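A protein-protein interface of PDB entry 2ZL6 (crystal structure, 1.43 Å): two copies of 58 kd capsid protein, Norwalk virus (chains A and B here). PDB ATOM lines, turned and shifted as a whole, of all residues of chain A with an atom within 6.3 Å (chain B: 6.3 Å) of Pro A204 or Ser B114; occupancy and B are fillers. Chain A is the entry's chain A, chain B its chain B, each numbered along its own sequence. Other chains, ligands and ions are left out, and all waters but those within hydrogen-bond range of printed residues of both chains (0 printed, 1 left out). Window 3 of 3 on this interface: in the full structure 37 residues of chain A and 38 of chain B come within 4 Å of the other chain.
No position is printed for both chains.
Of the 12 pairs that touch across the chains among the printed residues, none has its exchanged pair printed and touching as well.
Of chain B, only Gly B112 (3.7 Å), His B113 (3.5 Å) and Ser B114 (3.1 Å) come within 4 Å of Pro A204.
Of chain A, only Trp A151 (3.7 Å) and Pro A204 (3.1 Å) come within 4 Å of Ser B114.
Of the printed residues of chain A, Ser B115 touches Trp A151.
Of the printed residues of chain A, Gln B116 touches Trp A151 (3.7 Å).
Of the printed residues of chain A, Phe B111 touches Pro A202.
Tyr A207 touches none of the printed residues of chain B.
Ala A206 touches none of the printed residues of chain B.
The nearest residue of chain B that does not touch Pro A204 is Gln B110 (5.5 Å).
The nearest printed residue of chain A that does not touch His B113 is Gly A205 (4.7 Å).
Of the 11 printed residues of chain A, 5 touch a printed residue of chain B.
Printed residues of chain A that touch a printed residue of chain B: Trp A151, Pro A202, Gly A203, Pro A204 and Gly A205.
Hydrophobic or aromatic side chains of chain A within 4 Å of the printed part of chain B: Trp A151, Pro A202 and Pro A204.
Printed residues of chain B that touch a printed residue of chain A: Gln B110, Phe B111, Gly B112, His B113, Ser B114, Ser B115 and Gln B116.
Hydrophobic or aromatic side chains of chain B within 4 Å of the printed part of chain A: Phe B111.
O of Gly A203 lies within hydrogen-bond range of N of Gly B112 (2.9 Å).
The backbone nitrogen (N) of Pro A204 sits close to the backbone carbonyl oxygen (O) of His B113 (3.5 Å).
O of Gly A203 lies within hydrogen-bond range of N of His B113, at 3.2 Å.
The backbone NH (N) of Gly A203 sits at hydrogen-bond distance from the backbone carbonyl oxygen (O) of Gln B110 (3.1 Å).
Among the printed residues, merely in contact across the chains: Pro A204 with Ser B114 (3.1 Å), Trp A151 with Ser B115 (3.3 Å), Pro A202 with Gln B110 (3.5 Å), Pro A204 with Gly B112 (3.7 Å), Trp A151 with Gln B116 (3.7 Å), Trp A151 with Ser B114 (3.7 Å), Gly A205 with Gly B112 (3.7 Å) and Pro A202 with Phe B111 (3.9 Å).
The backbone NH (N) of Ile A152 is in hydrogen-bond range of the backbone carbonyl oxygen (O) of Pro A202 (3.1 Å).
The side-chain hydroxyl (OH) of Tyr A207 lies close to the backbone carbonyl oxygen (O) of Pro A204, at 3.4 Å.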
ATOM      1  N   TRP A 151      26.035   2.048   0.071  1.00  0.00           N
ATOM      2  CA  TRP A 151      25.515   2.351   1.404  1.00  0.00           C
ATOM      3  C   TRP A 151      26.659   2.885   2.240  1.00  0.00           C
ATOM      4  O   TRP A 151      27.827   2.756   1.856  1.00  0.00           O
ATOM      5  CB  TRP A 151      24.816   1.119   2.028  1.00  0.00           C
ATOM      6  CG  TRP A 151      25.704  -0.118   2.206  1.00  0.00           C
ATOM      7  CD1 TRP A 151      26.097  -0.991   1.233  1.00  0.00           C
ATOM      8  CD2 TRP A 151      26.296  -0.603   3.434  1.00  0.00           C
ATOM      9  NE1 TRP A 151      26.899  -1.975   1.768  1.00  0.00           N
ATOM     10  CE2 TRP A 151      27.035  -1.759   3.118  1.00  0.00           C
ATOM     11  CE3 TRP A 151      26.279  -0.159   4.763  1.00  0.00           C
ATOM     12  CZ2 TRP A 151      27.746  -2.482   4.084  1.00  0.00           C
ATOM     13  CZ3 TRP A 151      26.972  -0.882   5.722  1.00  0.00           C
ATOM     14  CH2 TRP A 151      27.698  -2.021   5.382  1.00  0.00           C
ATOM     15  N   ILE A 152      26.323   3.512   3.374  1.00  0.00           N
ATOM     16  CA  ILE A 152      27.352   4.060   4.265  1.00  0.00           C
ATOM     17  C   ILE A 152      27.152   3.562   5.694  1.00  0.00           C
ATOM     18  O   ILE A 152      26.107   3.013   6.027  1.00  0.00           O
ATOM     19  CB  ILE A 152      27.335   5.582   4.279  1.00  0.00           C
ATOM     20  CG1 ILE A 152      26.033   6.086   4.921  1.00  0.00           C
ATOM     21  CG2 ILE A 152      27.549   6.145   2.809  1.00  0.00           C
ATOM     22  CD1 ILE A 152      25.944   7.575   5.081  1.00  0.00           C
ATOM     23  N   SER A 153      28.196   3.725   6.502  1.00  0.00           N
ATOM     24  CA  SER A 153      28.119   3.350   7.916  1.00  0.00           C
ATOM     25  C   SER A 153      28.979   4.354   8.703  1.00  0.00           C
ATOM     26  O   SER A 153      29.688   5.204   8.125  1.00  0.00           O
ATOM     27  CB  SER A 153      28.586   1.901   8.091  1.00  0.00           C
ATOM     28  OG  SER A 153      29.917   1.739   7.641  1.00  0.00           O
ATOM     29  N   PRO A 154      28.906   4.301  10.049  1.00  0.00           N
ATOM     30  CA  PRO A 154      29.723   5.234  10.822  1.00  0.00           C
ATOM     31  C   PRO A 154      31.220   5.135  10.469  1.00  0.00           C
ATOM     32  O   PRO A 154      31.697   4.059  10.137  1.00  0.00           O
ATOM     33  CB  PRO A 154      29.493   4.774  12.275  1.00  0.00           C
ATOM     34  CG  PRO A 154      28.106   4.196  12.255  1.00  0.00           C
ATOM     35  CD  PRO A 154      28.059   3.451  10.916  1.00  0.00           C
ATOM     36  N   MET A 201      19.934   8.027   2.766  1.00  0.00           N
ATOM     37  CA  MET A 201      21.031   7.174   2.284  1.00  0.00           C
ATOM     38  C   MET A 201      20.976   5.837   3.005  1.00  0.00           C
ATOM     39  O   MET A 201      20.963   5.800   4.246  1.00  0.00           O
ATOM     40  CB  MET A 201      22.399   7.844   2.520  1.00  0.00           C
ATOM     41  CG  MET A 201      23.612   6.912   2.323  1.00  0.00           C
ATOM     42  SD  MET A 201      23.840   6.328   0.629  1.00  0.00           S
ATOM     43  CE  MET A 201      24.391   7.821  -0.049  1.00  0.00           C
ATOM     44  N   PRO A 202      20.914   4.714   2.261  1.00  0.00           N
ATOM     45  CA  PRO A 202      20.940   3.369   2.848  1.00  0.00           C
ATOM     46  C   PRO A 202      22.129   3.120   3.784  1.00  0.00           C
ATOM     47  O   PRO A 202      23.220   3.680   3.602  1.00  0.00           O
ATOM     48  CB  PRO A 202      20.980   2.447   1.608  1.00  0.00           C
ATOM     49  CG  PRO A 202      20.293   3.283   0.552  1.00  0.00           C
ATOM     50  CD  PRO A 202      20.727   4.675   0.789  1.00  0.00           C
ATOM     51  N   GLY A 203      21.866   2.299   4.800  1.00  0.00           N
ATOM     52  CA  GLY A 203      22.860   1.877   5.769  1.00  0.00           C
ATOM     53  C   GLY A 203      22.205   1.785   7.135  1.00  0.00           C
ATOM     54  O   GLY A 203      21.008   2.079   7.255  1.00  0.00           O
ATOM     55  N   PRO A 204      22.994   1.370   8.163  1.00  0.00           N
ATOM     56  CA  PRO A 204      22.465   1.008   9.505  1.00  0.00           C
ATOM     57  C   PRO A 204      22.105   2.200  10.390  1.00  0.00           C
ATOM     58  O   PRO A 204      22.506   2.254  11.574  1.00  0.00           O
ATOM     59  CB  PRO A 204      23.600   0.187  10.119  1.00  0.00           C
ATOM     60  CG  PRO A 204      24.843   0.741   9.472  1.00  0.00           C
ATOM     61  CD  PRO A 204      24.447   1.126   8.054  1.00  0.00           C
ATOM     62  N   GLY A 205      21.367   3.149   9.837  1.00  0.00           N
ATOM     63  CA  GLY A 205      20.894   4.320  10.586  1.00  0.00           C
ATOM     64  C   GLY A 205      19.960   5.159   9.749  1.00  0.00           C
ATOM     65  O   GLY A 205      19.667   4.814   8.592  1.00  0.00           O
ATOM     66  N   ALA A 206      19.497   6.266  10.314  1.00  0.00           N
ATOM     67  CA  ALA A 206      18.643   7.198   9.608  1.00  0.00           C
ATOM     68  C   ALA A 206      19.589   8.267   9.097  1.00  0.00           C
ATOM     69  O   ALA A 206      19.971   9.216   9.818  1.00  0.00           O
ATOM     70  CB  ALA A 206      17.563   7.795  10.547  1.00  0.00           C
ATOM     71  N   TYR A 207      20.055   8.075   7.867  1.00  0.00           N
ATOM     72  CA  TYR A 207      21.095   8.941   7.338  1.00  0.00           C
ATOM     73  C   TYR A 207      20.556   9.947   6.351  1.00  0.00           C
ATOM     74  O   TYR A 207      19.868   9.570   5.389  1.00  0.00           O
ATOM     75  CB  TYR A 207      22.197   8.125   6.690  1.00  0.00           C
ATOM     76  CG  TYR A 207      22.851   7.120   7.601  1.00  0.00           C
ATOM     77  CD1 TYR A 207      23.121   7.410   8.948  1.00  0.00           C
ATOM     78  CD2 TYR A 207      23.237   5.891   7.114  1.00  0.00           C
ATOM     79  CE1 TYR A 207      23.737   6.484   9.759  1.00  0.00           C
ATOM     80  CE2 TYR A 207      23.886   4.950   7.909  1.00  0.00           C
ATOM     81  CZ  TYR A 207      24.121   5.243   9.250  1.00  0.00           C
ATOM     82  OH  TYR A 207      24.756   4.281  10.033  1.00  0.00           O
ATOM     83  N   GLN B 110      19.188  -1.362   2.072  1.00  0.00           N
ATOM     84  CA  GLN B 110      18.074  -1.073   2.982  1.00  0.00           C
ATOM     85  C   GLN B 110      18.242   0.211   3.774  1.00  0.00           C
ATOM     86  O   GLN B 110      19.359   0.576   4.162  1.00  0.00           O
ATOM     87  CB  GLN B 110      17.912  -2.234   3.972  1.00  0.00           C
ATOM     88  CG  GLN B 110      17.632  -3.541   3.299  1.00  0.00           C
ATOM     89  CD  GLN B 110      17.366  -4.649   4.271  1.00  0.00           C
ATOM     90  OE1 GLN B 110      18.293  -5.191   4.873  1.00  0.00           O
ATOM     91  NE2 GLN B 110      16.087  -5.007   4.418  1.00  0.00           N
ATOM     92  N   PHE B 111      17.128   0.890   4.028  1.00  0.00           N
ATOM     93  CA  PHE B 111      17.135   2.008   4.948  1.00  0.00           C
ATOM     94  C   PHE B 111      17.076   1.515   6.386  1.00  0.00           C
ATOM     95  O   PHE B 111      16.081   0.923   6.803  1.00  0.00           O
ATOM     96  CB  PHE B 111      15.987   2.953   4.655  1.00  0.00           C
ATOM     97  CG  PHE B 111      16.010   3.477   3.254  1.00  0.00           C
ATOM     98  CD1 PHE B 111      16.927   4.468   2.878  1.00  0.00           C
ATOM     99  CD2 PHE B 111      15.171   2.928   2.286  1.00  0.00           C
ATOM    100  CE1 PHE B 111      16.959   4.958   1.567  1.00  0.00           C
ATOM    101  CE2 PHE B 111      15.203   3.404   0.963  1.00  0.00           C
ATOM    102  CZ  PHE B 111      16.110   4.425   0.608  1.00  0.00           C
ATOM    103  N   GLY B 112      18.177   1.717   7.101  1.00  0.00           N
ATOM    104  CA  GLY B 112      18.273   1.319   8.510  1.00  0.00           C
ATOM    105  C   GLY B 112      18.959  -0.010   8.761  1.00  0.00           C
ATOM    106  O   GLY B 112      18.997  -0.477   9.902  1.00  0.00           O
ATOM    107  N   HIS B 113      19.496  -0.653   7.718  1.00  0.00           N
ATOM    108  CA  HIS B 113      20.287  -1.871   7.894  1.00  0.00           C
ATOM    109  C   HIS B 113      21.563  -1.790   7.094  1.00  0.00           C
ATOM    110  O   HIS B 113      21.618  -1.080   6.079  1.00  0.00           O
ATOM    111  CB  HIS B 113      19.518  -3.127   7.473  1.00  0.00           C
ATOM    112  CG  HIS B 113      18.248  -3.323   8.235  1.00  0.00           C
ATOM    113  ND1 HIS B 113      18.215  -3.894   9.489  1.00  0.00           N
ATOM    114  CD2 HIS B 113      16.968  -3.010   7.926  1.00  0.00           C
ATOM    115  CE1 HIS B 113      16.966  -3.930   9.917  1.00  0.00           C
ATOM    116  NE2 HIS B 113      16.190  -3.397   8.990  1.00  0.00           N
ATOM    117  N   SER B 114      22.572  -2.516   7.571  1.00  0.00           N
ATOM    118  CA  SER B 114      23.836  -2.636   6.857  1.00  0.00           C
ATOM    119  C   SER B 114      23.702  -3.584   5.673  1.00  0.00           C
ATOM    120  O   SER B 114      22.704  -4.294   5.538  1.00  0.00           O
ATOM    121  CB  SER B 114      24.899  -3.196   7.789  1.00  0.00           C
ATOM    122  OG  SER B 114      25.170  -2.288   8.831  1.00  0.00           O
ATOM    123  N   SER B 115      24.749  -3.614   4.837  1.00  0.00           N
ATOM    124  CA  SER B 115      24.950  -4.633   3.797  1.00  0.00           C
ATOM    125  C   SER B 115      24.243  -4.364   2.471  1.00  0.00           C
ATOM    126  O   SER B 115      23.270  -3.621   2.402  1.00  0.00           O
ATOM    127  CB  SER B 115      24.549  -6.024   4.303  1.00  0.00           C
ATOM    128  OG  SER B 115      25.077  -6.262   5.595  1.00  0.00           O
ATOM    129  N   GLN B 116      24.764  -5.015   1.436  1.00  0.00           N
ATOM    130  CA  GLN B 116      24.077  -5.089   0.150  1.00  0.00           C
ATOM    131  C   GLN B 116      23.942  -6.563  -0.223  1.00  0.00           C
ATOM    132  O   GLN B 116      24.700  -7.403   0.264  1.00  0.00           O
ATOM    133  CB  GLN B 116      24.876  -4.344  -0.929  1.00  0.00           C
ATOM    134  CG  GLN B 116      26.254  -4.965  -1.220  1.00  0.00           C
ATOM    135  CD  GLN B 116      27.044  -4.230  -2.321  1.00  0.00           C
ATOM    136  OE1 GLN B 116      27.833  -4.843  -3.056  1.00  0.00           O
ATOM    137  NE2 GLN B 116      26.859  -2.936  -2.411  1.00  0.00           N
